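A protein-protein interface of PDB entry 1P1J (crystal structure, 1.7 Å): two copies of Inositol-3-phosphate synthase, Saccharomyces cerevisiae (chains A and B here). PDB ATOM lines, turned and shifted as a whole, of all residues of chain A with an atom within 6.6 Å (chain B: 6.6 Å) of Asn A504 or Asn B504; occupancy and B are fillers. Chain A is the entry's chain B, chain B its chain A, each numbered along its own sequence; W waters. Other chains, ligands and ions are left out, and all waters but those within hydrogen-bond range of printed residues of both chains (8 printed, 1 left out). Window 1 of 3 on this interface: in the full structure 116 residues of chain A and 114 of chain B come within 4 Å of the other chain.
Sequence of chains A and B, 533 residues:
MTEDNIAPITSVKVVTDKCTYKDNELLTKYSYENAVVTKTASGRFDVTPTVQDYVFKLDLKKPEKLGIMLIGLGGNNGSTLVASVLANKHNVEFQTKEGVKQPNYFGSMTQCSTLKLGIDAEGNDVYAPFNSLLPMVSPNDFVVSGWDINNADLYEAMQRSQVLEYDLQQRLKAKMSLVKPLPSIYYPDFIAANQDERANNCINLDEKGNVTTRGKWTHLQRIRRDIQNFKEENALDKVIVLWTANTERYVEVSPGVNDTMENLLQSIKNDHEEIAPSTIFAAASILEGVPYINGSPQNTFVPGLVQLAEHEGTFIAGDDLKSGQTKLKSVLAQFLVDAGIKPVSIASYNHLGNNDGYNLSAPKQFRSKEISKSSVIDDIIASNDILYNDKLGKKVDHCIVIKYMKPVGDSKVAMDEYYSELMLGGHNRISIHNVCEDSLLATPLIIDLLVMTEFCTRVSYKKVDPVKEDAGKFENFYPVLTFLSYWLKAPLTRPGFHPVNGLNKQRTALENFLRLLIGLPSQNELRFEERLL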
ATOM      1  N   SER A 330     -27.862   2.969   3.452  1.00  0.00           N
ATOM      2  CA  SER A 330     -27.050   2.772   4.658  1.00  0.00           C
ATOM      3  C   SER A 330     -27.824   3.171   5.912  1.00  0.00           C
ATOM      4  O   SER A 330     -27.336   3.020   7.038  1.00  0.00           O
ATOM      5  CB  SER A 330     -25.736   3.571   4.572  1.00  0.00           C
ATOM      6  OG  SER A 330     -25.964   4.969   4.610  1.00  0.00           O
ATOM      7  N   VAL A 331     -29.032   3.690   5.704  1.00  0.00           N
ATOM      8  CA  VAL A 331     -29.910   4.076   6.800  1.00  0.00           C
ATOM      9  C   VAL A 331     -31.056   3.065   6.894  1.00  0.00           C
ATOM     10  O   VAL A 331     -31.311   2.500   7.954  1.00  0.00           O
ATOM     11  CB  VAL A 331     -30.514   5.485   6.586  1.00  0.00           C
ATOM     12  CG1 VAL A 331     -31.577   5.758   7.645  1.00  0.00           C
ATOM     13  CG2 VAL A 331     -29.418   6.544   6.671  1.00  0.00           C
ATOM     14  N   GLN A 334     -30.046  -0.768   7.625  1.00  0.00           N
ATOM     15  CA  GLN A 334     -29.616  -0.844   9.018  1.00  0.00           C
ATOM     16  C   GLN A 334     -30.827  -0.818   9.953  1.00  0.00           C
ATOM     17  O   GLN A 334     -30.907  -1.590  10.912  1.00  0.00           O
ATOM     18  CB  GLN A 334     -28.696   0.332   9.345  1.00  0.00           C
ATOM     19  CG  GLN A 334     -28.029   0.233  10.715  1.00  0.00           C
ATOM     20  CD  GLN A 334     -26.953  -0.836  10.759  1.00  0.00           C
ATOM     21  OE1 GLN A 334     -27.106  -1.873  11.413  1.00  0.00           O
ATOM     22  NE2 GLN A 334     -25.855  -0.589  10.055  1.00  0.00           N
ATOM     23  N   PHE A 335     -31.764   0.076   9.660  1.00  0.00           N
ATOM     24  CA  PHE A 335     -32.984   0.225  10.447  1.00  0.00           C
ATOM     25  C   PHE A 335     -33.779  -1.082  10.498  1.00  0.00           C
ATOM     26  O   PHE A 335     -34.198  -1.534  11.574  1.00  0.00           O
ATOM     27  CB  PHE A 335     -33.818   1.372   9.843  1.00  0.00           C
ATOM     28  CG  PHE A 335     -35.310   1.189   9.943  1.00  0.00           C
ATOM     29  CD1 PHE A 335     -36.108   1.330   8.805  1.00  0.00           C
ATOM     30  CD2 PHE A 335     -35.925   0.913  11.159  1.00  0.00           C
ATOM     31  CE1 PHE A 335     -37.496   1.200   8.881  1.00  0.00           C
ATOM     32  CE2 PHE A 335     -37.311   0.782  11.244  1.00  0.00           C
ATOM     33  CZ  PHE A 335     -38.096   0.925  10.106  1.00  0.00           C
ATOM     34  N   ASP A 338     -31.861  -3.814  12.504  1.00  0.00           N
ATOM     35  CA  ASP A 338     -31.796  -3.437  13.915  1.00  0.00           C
ATOM     36  C   ASP A 338     -33.150  -3.696  14.579  1.00  0.00           C
ATOM     37  O   ASP A 338     -33.232  -3.897  15.792  1.00  0.00           O
ATOM     38  CB  ASP A 338     -31.447  -1.953  14.066  1.00  0.00           C
ATOM     39  CG  ASP A 338     -29.976  -1.655  13.799  1.00  0.00           C
ATOM     40  OD1 ASP A 338     -29.598  -0.466  13.887  1.00  0.00           O
ATOM     41  OD2 ASP A 338     -29.201  -2.594  13.510  1.00  0.00           O
ATOM     42  N   TYR A 486     -18.677   8.428   6.799  1.00  0.00           N
ATOM     43  CA  TYR A 486     -20.033   8.957   6.673  1.00  0.00           C
ATOM     44  C   TYR A 486     -20.324   9.435   5.254  1.00  0.00           C
ATOM     45  O   TYR A 486     -21.453   9.335   4.765  1.00  0.00           O
ATOM     46  CB  TYR A 486     -20.222  10.137   7.635  1.00  0.00           C
ATOM     47  CG  TYR A 486     -21.562  10.839   7.512  1.00  0.00           C
ATOM     48  CD1 TYR A 486     -22.658  10.447   8.290  1.00  0.00           C
ATOM     49  CD2 TYR A 486     -21.745  11.875   6.594  1.00  0.00           C
ATOM     50  CE1 TYR A 486     -23.903  11.072   8.152  1.00  0.00           C
ATOM     51  CE2 TYR A 486     -22.983  12.502   6.446  1.00  0.00           C
ATOM     52  CZ  TYR A 486     -24.057  12.096   7.226  1.00  0.00           C
ATOM     53  OH  TYR A 486     -25.277  12.718   7.066  1.00  0.00           O
ATOM     54  N   ASN A 501     -20.607   0.342   7.462  1.00  0.00           N
ATOM     55  CA  ASN A 501     -21.351   1.226   6.568  1.00  0.00           C
ATOM     56  C   ASN A 501     -22.570   1.971   7.103  1.00  0.00           C
ATOM     57  O   ASN A 501     -23.056   2.902   6.450  1.00  0.00           O
ATOM     58  CB  ASN A 501     -21.745   0.430   5.322  1.00  0.00           C
ATOM     59  CG  ASN A 501     -20.540  -0.005   4.514  1.00  0.00           C
ATOM     60  OD1 ASN A 501     -19.810   0.830   3.980  1.00  0.00           O
ATOM     61  ND2 ASN A 501     -20.317  -1.312   4.427  1.00  0.00           N
ATOM     62  N   GLY A 502     -23.064   1.575   8.272  1.00  0.00           N
ATOM     63  CA  GLY A 502     -24.224   2.237   8.844  1.00  0.00           C
ATOM     64  C   GLY A 502     -23.997   3.728   9.020  1.00  0.00           C
ATOM     65  O   GLY A 502     -23.102   4.144   9.753  1.00  0.00           O
ATOM     66  N   LEU A 503     -24.817   4.536   8.357  1.00  0.00           N
ATOM     67  CA  LEU A 503     -24.684   5.985   8.421  1.00  0.00           C
ATOM     68  C   LEU A 503     -24.731   6.554   9.835  1.00  0.00           C
ATOM     69  O   LEU A 503     -23.881   7.360  10.215  1.00  0.00           O
ATOM     70  CB  LEU A 503     -25.773   6.660   7.581  1.00  0.00           C
ATOM     71  CG  LEU A 503     -25.491   8.132   7.265  1.00  0.00           C
ATOM     72  CD1 LEU A 503     -24.394   8.213   6.211  1.00  0.00           C
ATOM     73  CD2 LEU A 503     -26.747   8.820   6.764  1.00  0.00           C
ATOM     74  N   ASN A 504     -25.726   6.148  10.613  1.00  0.00           N
ATOM     75  CA  ASN A 504     -25.848   6.670  11.967  1.00  0.00           C
ATOM     76  C   ASN A 504     -24.627   6.366  12.833  1.00  0.00           C
ATOM     77  O   ASN A 504     -24.180   7.224  13.592  1.00  0.00           O
ATOM     78  CB  ASN A 504     -27.130   6.143  12.607  1.00  0.00           C
ATOM     79  CG  ASN A 504     -28.374   6.759  11.987  1.00  0.00           C
ATOM     80  OD1 ASN A 504     -29.477   6.242  12.139  1.00  0.00           O
ATOM     81  ND2 ASN A 504     -28.198   7.878  11.290  1.00  0.00           N
ATOM     82  N   LYS A 505     -24.076   5.165  12.710  1.00  0.00           N
ATOM     83  CA  LYS A 505     -22.890   4.815  13.489  1.00  0.00           C
ATOM     84  C   LYS A 505     -21.705   5.650  13.020  1.00  0.00           C
ATOM     85  O   LYS A 505     -20.845   6.031  13.813  1.00  0.00           O
ATOM     86  CB  LYS A 505     -22.569   3.332  13.349  1.00  0.00           C
ATOM     87  CG  LYS A 505     -23.527   2.439  14.123  1.00  0.00           C
ATOM     88  CD  LYS A 505     -23.131   0.983  14.043  1.00  0.00           C
ATOM     89  CE  LYS A 505     -23.321   0.428  12.649  1.00  0.00           C
ATOM     90  NZ  LYS A 505     -22.996  -1.021  12.617  1.00  0.00           N
ATOM     91  N   GLN A 506     -21.669   5.937  11.722  1.00  0.00           N
ATOM     92  CA  GLN A 506     -20.593   6.741  11.160  1.00  0.00           C
ATOM     93  C   GLN A 506     -20.670   8.184  11.663  1.00  0.00           C
ATOM     94  O   GLN A 506     -19.640   8.815  11.908  1.00  0.00           O
ATOM     95  CB  GLN A 506     -20.654   6.692   9.627  1.00  0.00           C
ATOM     96  CG  GLN A 506     -20.264   5.328   9.053  1.00  0.00           C
ATOM     97  CD  GLN A 506     -20.524   5.215   7.558  1.00  0.00           C
ATOM     98  OE1 GLN A 506     -19.950   4.360   6.882  1.00  0.00           O
ATOM     99  NE2 GLN A 506     -21.398   6.066   7.041  1.00  0.00           N
ATOM    100  N   ARG A 507     -21.881   8.714  11.824  1.00  0.00           N
ATOM    101  CA  ARG A 507     -22.007  10.076  12.325  1.00  0.00           C
ATOM    102  C   ARG A 507     -21.726  10.069  13.823  1.00  0.00           C
ATOM    103  O   ARG A 507     -21.132  11.006  14.352  1.00  0.00           O
ATOM    104  CB  ARG A 507     -23.403  10.650  12.055  1.00  0.00           C
ATOM    105  CG  ARG A 507     -23.532  12.113  12.471  1.00  0.00           C
ATOM    106  CD  ARG A 507     -24.740  12.786  11.830  1.00  0.00           C
ATOM    107  NE  ARG A 507     -24.779  14.221  12.098  1.00  0.00           N
ATOM    108  CZ  ARG A 507     -25.325  14.776  13.176  1.00  0.00           C
ATOM    109  NH1 ARG A 507     -25.306  16.095  13.319  1.00  0.00           N
ATOM    110  NH2 ARG A 507     -25.899  14.022  14.107  1.00  0.00           N
ATOM    111  N   THR A 508     -22.151   9.006  14.502  1.00  0.00           N
ATOM    112  CA  THR A 508     -21.914   8.887  15.937  1.00  0.00           C
ATOM    113  C   THR A 508     -20.410   8.919  16.222  1.00  0.00           C
ATOM    114  O   THR A 508     -19.967   9.569  17.170  1.00  0.00           O
ATOM    115  CB  THR A 508     -22.526   7.583  16.497  1.00  0.00           C
ATOM    116  OG1 THR A 508     -23.953   7.712  16.544  1.00  0.00           O
ATOM    117  CG2 THR A 508     -22.003   7.299  17.906  1.00  0.00           C
ATOM    118  N   ALA A 509     -19.634   8.225  15.396  1.00  0.00           N
ATOM    119  CA  ALA A 509     -18.180   8.191  15.556  1.00  0.00           C
ATOM    120  C   ALA A 509     -17.599   9.606  15.521  1.00  0.00           C
ATOM    121  O   ALA A 509     -16.796   9.978  16.376  1.00  0.00           O
ATOM    122  CB  ALA A 509     -17.553   7.341  14.457  1.00  0.00           C
ATOM    123  N   GLU A 525     -27.760   8.573  25.646  1.00  0.00           N
ATOM    124  CA  GLU A 525     -29.221   8.596  25.575  1.00  0.00           C
ATOM    125  C   GLU A 525     -29.930   7.944  26.759  1.00  0.00           C
ATOM    126  O   GLU A 525     -31.114   7.610  26.667  1.00  0.00           O
ATOM    127  CB  GLU A 525     -29.695   7.925  24.279  1.00  0.00           C
ATOM    128  CG  GLU A 525     -29.481   8.761  23.030  1.00  0.00           C
ATOM    129  CD  GLU A 525     -30.239  10.073  23.079  1.00  0.00           C
ATOM    130  OE1 GLU A 525     -31.459  10.049  23.356  1.00  0.00           O
ATOM    131  OE2 GLU A 525     -29.621  11.129  22.838  1.00  0.00           O
ATOM    132  N   SER B 330     -39.740   8.140  11.704  1.00  0.00           N
ATOM    133  CA  SER B 330     -38.858   8.455  12.829  1.00  0.00           C
ATOM    134  C   SER B 330     -37.411   8.091  12.507  1.00  0.00           C
ATOM    135  O   SER B 330     -36.504   8.347  13.304  1.00  0.00           O
ATOM    136  CB  SER B 330     -39.316   7.748  14.120  1.00  0.00           C
ATOM    137  OG  SER B 330     -39.103   6.349  14.084  1.00  0.00           O
ATOM    138  N   VAL B 331     -37.210   7.485  11.339  1.00  0.00           N
ATOM    139  CA  VAL B 331     -35.878   7.116  10.865  1.00  0.00           C
ATOM    140  C   VAL B 331     -35.459   8.079   9.749  1.00  0.00           C
ATOM    141  O   VAL B 331     -34.365   8.648   9.779  1.00  0.00           O
ATOM    142  CB  VAL B 331     -35.847   5.675  10.287  1.00  0.00           C
ATOM    143  CG1 VAL B 331     -34.529   5.429   9.560  1.00  0.00           C
ATOM    144  CG2 VAL B 331     -36.031   4.658  11.400  1.00  0.00           C
ATOM    145  N   GLN B 334     -35.245  11.997  10.741  1.00  0.00           N
ATOM    146  CA  GLN B 334     -34.069  12.177  11.582  1.00  0.00           C
ATOM    147  C   GLN B 334     -32.811  12.174  10.716  1.00  0.00           C
ATOM    148  O   GLN B 334     -31.927  13.018  10.872  1.00  0.00           O
ATOM    149  CB  GLN B 334     -33.991  11.051  12.617  1.00  0.00           C
ATOM    150  CG  GLN B 334     -32.914  11.250  13.679  1.00  0.00           C
ATOM    151  CD  GLN B 334     -33.254  12.366  14.646  1.00  0.00           C
ATOM    152  OE1 GLN B 334     -32.606  13.420  14.664  1.00  0.00           O
ATOM    153  NE2 GLN B 334     -34.281  12.145  15.457  1.00  0.00           N
ATOM    154  N   PHE B 335     -32.750  11.222   9.792  1.00  0.00           N
ATOM    155  CA  PHE B 335     -31.620  11.095   8.883  1.00  0.00           C
ATOM    156  C   PHE B 335     -31.401  12.368   8.059  1.00  0.00           C
ATOM    157  O   PHE B 335     -30.280  12.883   7.985  1.00  0.00           O
ATOM    158  CB  PHE B 335     -31.852   9.866   7.986  1.00  0.00           C
ATOM    159  CG  PHE B 335     -31.281   9.981   6.604  1.00  0.00           C
ATOM    160  CD1 PHE B 335     -29.921  10.194   6.406  1.00  0.00           C
ATOM    161  CD2 PHE B 335     -32.109   9.858   5.491  1.00  0.00           C
ATOM    162  CE1 PHE B 335     -29.396  10.283   5.122  1.00  0.00           C
ATOM    163  CE2 PHE B 335     -31.592   9.944   4.203  1.00  0.00           C
ATOM    164  CZ  PHE B 335     -30.230  10.158   4.021  1.00  0.00           C
ATOM    165  N   ASP B 338     -30.252  15.273  10.342  1.00  0.00           N
ATOM    166  CA  ASP B 338     -28.911  14.999  10.861  1.00  0.00           C
ATOM    167  C   ASP B 338     -27.872  15.251   9.767  1.00  0.00           C
ATOM    168  O   ASP B 338     -26.713  15.549  10.060  1.00  0.00           O
ATOM    169  CB  ASP B 338     -28.789  13.543  11.324  1.00  0.00           C
ATOM    170  CG  ASP B 338     -29.466  13.283  12.667  1.00  0.00           C
ATOM    171  OD1 ASP B 338     -29.421  12.122  13.124  1.00  0.00           O
ATOM    172  OD2 ASP B 338     -30.031  14.223  13.265  1.00  0.00           O
ATOM    173  N   TYR B 486     -39.099   3.370  21.865  1.00  0.00           N
ATOM    174  CA  TYR B 486     -38.786   2.781  20.563  1.00  0.00           C
ATOM    175  C   TYR B 486     -40.033   2.220  19.886  1.00  0.00           C
ATOM    176  O   TYR B 486     -40.172   2.265  18.665  1.00  0.00           O
ATOM    177  CB  TYR B 486     -37.755   1.653  20.741  1.00  0.00           C
ATOM    178  CG  TYR B 486     -37.436   0.870  19.477  1.00  0.00           C
ATOM    179  CD1 TYR B 486     -38.237  -0.200  19.067  1.00  0.00           C
ATOM    180  CD2 TYR B 486     -36.344   1.218  18.676  1.00  0.00           C
ATOM    181  CE1 TYR B 486     -37.964  -0.902  17.889  1.00  0.00           C
ATOM    182  CE2 TYR B 486     -36.061   0.522  17.491  1.00  0.00           C
ATOM    183  CZ  TYR B 486     -36.875  -0.533  17.104  1.00  0.00           C
ATOM    184  OH  TYR B 486     -36.617  -1.206  15.927  1.00  0.00           O
ATOM    185  N   ASN B 501     -38.224  11.401  19.684  1.00  0.00           N
ATOM    186  CA  ASN B 501     -38.781  10.407  18.771  1.00  0.00           C
ATOM    187  C   ASN B 501     -37.846   9.638  17.838  1.00  0.00           C
ATOM    188  O   ASN B 501     -38.256   8.623  17.268  1.00  0.00           O
ATOM    189  CB  ASN B 501     -39.883  11.066  17.937  1.00  0.00           C
ATOM    190  CG  ASN B 501     -41.028  11.588  18.792  1.00  0.00           C
ATOM    191  OD1 ASN B 501     -41.211  12.797  18.948  1.00  0.00           O
ATOM    192  ND2 ASN B 501     -41.799  10.674  19.357  1.00  0.00           N
ATOM    193  N   GLY B 502     -36.611  10.104  17.669  1.00  0.00           N
ATOM    194  CA  GLY B 502     -35.686   9.414  16.782  1.00  0.00           C
ATOM    195  C   GLY B 502     -35.533   7.947  17.139  1.00  0.00           C
ATOM    196  O   GLY B 502     -35.087   7.621  18.242  1.00  0.00           O
ATOM    197  N   LEU B 503     -35.886   7.063  16.208  1.00  0.00           N
ATOM    198  CA  LEU B 503     -35.817   5.625  16.452  1.00  0.00           C
ATOM    199  C   LEU B 503     -34.444   5.128  16.878  1.00  0.00           C
ATOM    200  O   LEU B 503     -34.326   4.350  17.818  1.00  0.00           O
ATOM    201  CB  LEU B 503     -36.258   4.835  15.214  1.00  0.00           C
ATOM    202  CG  LEU B 503     -36.546   3.353  15.500  1.00  0.00           C
ATOM    203  CD1 LEU B 503     -37.883   3.234  16.219  1.00  0.00           C
ATOM    204  CD2 LEU B 503     -36.593   2.553  14.202  1.00  0.00           C
ATOM    205  N   ASN B 504     -33.400   5.569  16.190  1.00  0.00           N
ATOM    206  CA  ASN B 504     -32.073   5.097  16.546  1.00  0.00           C
ATOM    207  C   ASN B 504     -31.629   5.533  17.933  1.00  0.00           C
ATOM    208  O   ASN B 504     -30.978   4.763  18.637  1.00  0.00           O
ATOM    209  CB  ASN B 504     -31.073   5.501  15.469  1.00  0.00           C
ATOM    210  CG  ASN B 504     -31.330   4.769  14.164  1.00  0.00           C
ATOM    211  OD1 ASN B 504     -31.447   3.541  14.144  1.00  0.00           O
ATOM    212  ND2 ASN B 504     -31.432   5.513  13.075  1.00  0.00           N
ATOM    213  N   LYS B 505     -31.994   6.744  18.343  1.00  0.00           N
ATOM    214  CA  LYS B 505     -31.633   7.199  19.686  1.00  0.00           C
ATOM    215  C   LYS B 505     -32.398   6.374  20.719  1.00  0.00           C
ATOM    216  O   LYS B 505     -31.869   6.053  21.784  1.00  0.00           O
ATOM    217  CB  LYS B 505     -31.957   8.684  19.866  1.00  0.00           C
ATOM    218  CG  LYS B 505     -30.956   9.595  19.180  1.00  0.00           C
ATOM    219  CD  LYS B 505     -31.246  11.058  19.435  1.00  0.00           C
ATOM    220  CE  LYS B 505     -32.526  11.503  18.768  1.00  0.00           C
ATOM    221  NZ  LYS B 505     -32.738  12.966  18.944  1.00  0.00           N
ATOM    222  N   GLN B 506     -33.643   6.029  20.399  1.00  0.00           N
ATOM    223  CA  GLN B 506     -34.460   5.231  21.307  1.00  0.00           C
ATOM    224  C   GLN B 506     -33.874   3.831  21.471  1.00  0.00           C
ATOM    225  O   GLN B 506     -33.904   3.268  22.564  1.00  0.00           O
ATOM    226  CB  GLN B 506     -35.906   5.150  20.799  1.00  0.00           C
ATOM    227  CG  GLN B 506     -36.581   6.510  20.711  1.00  0.00           C
ATOM    228  CD  GLN B 506     -37.927   6.460  20.019  1.00  0.00           C
ATOM    229  OE1 GLN B 506     -38.141   5.652  19.116  1.00  0.00           O
ATOM    230  NE2 GLN B 506     -38.835   7.342  20.422  1.00  0.00           N
ATOM    231  N   ARG B 507     -33.331   3.261  20.398  1.00  0.00           N
ATOM    232  CA  ARG B 507     -32.746   1.929  20.517  1.00  0.00           C
ATOM    233  C   ARG B 507     -31.405   2.006  21.241  1.00  0.00           C
ATOM    234  O   ARG B 507     -31.058   1.110  22.010  1.00  0.00           O
ATOM    235  CB  ARG B 507     -32.563   1.273  19.143  1.00  0.00           C
ATOM    236  CG  ARG B 507     -32.010  -0.142  19.235  1.00  0.00           C
ATOM    237  CD  ARG B 507     -32.238  -0.913  17.946  1.00  0.00           C
ATOM    238  NE  ARG B 507     -31.920  -2.330  18.088  1.00  0.00           N
ATOM    239  CZ  ARG B 507     -30.705  -2.852  17.947  1.00  0.00           C
ATOM    240  NH1 ARG B 507     -29.671  -2.076  17.656  1.00  0.00           N
ATOM    241  NH2 ARG B 507     -30.528  -4.160  18.082  1.00  0.00           N
ATOM    242  N   THR B 508     -30.661   3.079  20.997  1.00  0.00           N
ATOM    243  CA  THR B 508     -29.362   3.272  21.637  1.00  0.00           C
ATOM    244  C   THR B 508     -29.541   3.336  23.155  1.00  0.00           C
ATOM    245  O   THR B 508     -28.733   2.785  23.906  1.00  0.00           O
ATOM    246  CB  THR B 508     -28.685   4.564  21.130  1.00  0.00           C
ATOM    247  OG1 THR B 508     -28.254   4.368  19.774  1.00  0.00           O
ATOM    248  CG2 THR B 508     -27.480   4.930  21.994  1.00  0.00           C
ATOM    249  N   ALA B 509     -30.606   3.999  23.596  1.00  0.00           N
ATOM    250  CA  ALA B 509     -30.898   4.117  25.026  1.00  0.00           C
ATOM    251  C   ALA B 509     -31.041   2.727  25.638  1.00  0.00           C
ATOM    252  O   ALA B 509     -30.443   2.424  26.671  1.00  0.00           O
ATOM    253  CB  ALA B 509     -32.179   4.914  25.237  1.00  0.00           C
ATOM    254  N   GLU B 525     -18.328   3.955  19.048  1.00  0.00           N
ATOM    255  CA  GLU B 525     -17.976   3.828  17.631  1.00  0.00           C
ATOM    256  C   GLU B 525     -16.673   4.553  17.279  1.00  0.00           C
ATOM    257  O   GLU B 525     -16.413   4.844  16.109  1.00  0.00           O
ATOM    258  CB  GLU B 525     -19.114   4.372  16.756  1.00  0.00           C
ATOM    259  CG  GLU B 525     -20.492   3.794  17.075  1.00  0.00           C
ATOM    260  CD  GLU B 525     -20.636   2.323  16.715  1.00  0.00           C
ATOM    261  OE1 GLU B 525     -21.677   1.724  17.066  1.00  0.00           O
ATOM    262  OE2 GLU B 525     -19.722   1.763  16.075  1.00  0.00           O
HETATM  263  O   HOH W   1     -34.632  -0.352  14.404  1.00  0.00           O
HETATM  264  O   HOH W   2     -27.440  11.795   8.488  1.00  0.00           O
HETATM  265  O   HOH W   3     -31.446  13.579  21.575  1.00  0.00           O
HETATM  266  O   HOH W   4     -30.359   0.703  16.186  1.00  0.00           O
HETATM  267  O   HOH W   5     -26.968  10.984  13.286  1.00  0.00           O
HETATM  268  O   HOH W   6     -30.762   1.702  12.590  1.00  0.00           O
HETATM  269  O   HOH W   7     -32.322   7.966  11.492  1.00  0.00           O
HETATM  270  O   HOH W   8     -30.286   9.723  11.669  1.00  0.00           O
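Water W6 lies within hydrogen-bond range of the side-chain amide oxygen (OD1) of Asn B504 (2.5 Å), the side-chain carboxylate (OD1) of Asp A338 (2.8 Å) and the backbone NH (N) of Phe A335 (3.5 Å). Water W4 lies within hydrogen-bond range of OD1 of Asp A338 (2.7 Å) and NH1 of Arg B507 (3.2 Å). Water W5 lies within hydrogen-bond range of the side-chain carboxylate of Asp B338 (2.7 Å) and the guanidinium group of Arg A507 (3.3 Å). Water W2 lies within hydrogen-bond range of OH of Tyr A486 (2.7 Å) and O of Phe B335 (3.1 Å). Water W7 lies within hydrogen-bond range of the backbone carbonyl oxygen of Val B331 (2.8 Å), the side-chain amide nitrogen of Asn B504 (3.1 Å) and the side-chain amide oxygen of Asn A504 (3.4 Å). Water W3 lies within hydrogen-bond range of the side-chain amino group (NZ) of Lys B505 and the side-chain carboxylate (OE2) of Glu A525.
The guanidinium group (NE) of Arg A507 sits at hydrogen-bond distance from the backbone carbonyl oxygen (O) of Asp B338, 3.1 Å away. NE of Arg B507 lies within hydrogen-bond range of O of Asp A338, at 3.1 Å. The side-chain amide nitrogen (ND2) of Asn B504 sits close to the side-chain amide oxygen (OD1) of Asn A504 (2.3 Å).
Val A331 touches Val B331 (CG1 to CG1, 3.5 Å). Val A331 touches Phe B335. Val B331 touches Phe A335. Leu B503 touches Phe A335. Leu A503 touches Phe B335. Lys A505 touches Glu B525. CG2 of Thr A508 touches CG of Glu B525 (3.9 Å). CB of Ala A509 touches O of Glu B525, at 3.2 Å. Lys B505 touches Glu A525 (CD to OE2, 3.8 Å). Ala B509 touches Glu A525 (CB to O, 3.2 Å).
Hydrophobic or aromatic side chains of chain B that line the printed part of chain A: Val B331, Phe B335, Leu B503 and Ala B509. Hydrophobic or aromatic side chains of chain A that line the printed part of chain B: Val A331, Phe A335, Leu A503 and Ala A509.
Asn A504 touches just one residue of chain B: Asn B504. Ser B330 touches none of the printed residues of chain A. Printed residues of chain A within 4 Å of Val B331: Val A331 and Phe A335. Of the printed residues of chain A, Phe B335 touches Val A331 (3.7 Å) and Leu A503 (3.4 Å). Gly B502 touches none of the printed residues of chain A. Asn B504 touches one residue of chain A. The nearest residue of chain A that does not touch Asn B504 is Asp A338 (4.4 Å).
Val A331 touches its own counterpart, Val B331. Asp A338 touches Arg B507, and with the chains exchanged Arg A507 touches Asp B338. Asn B504 touches its own counterpart, Asn A504. Thr A508 touches Glu B525, but with the chains exchanged Glu A525 does not touch Thr B508 (4.4 Å). 16 positions are printed for both chains.
The backbone NH (N) of Leu B503 is in hydrogen-bond range of the backbone carbonyl oxygen (O) of Ser B330 (3.2 Å). The side-chain amide oxygen (OE1) of Gln B334 lies close to the side-chain carboxylate (OD2) of Asp B338 (3.0 Å). OG1 of Thr B508 sits at hydrogen-bond distance from O of Asn B504. O of Ser A330 sits at hydrogen-bond distance from N of Leu A503. The side-chain amide oxygen (OE1) of Gln A334 sits close to the side-chain carboxylate (OD2) of Asp A338 (3.1 Å). OG1 of Thr A508 lies within hydrogen-bond range of O of Asn A504, at 3.0 Å.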
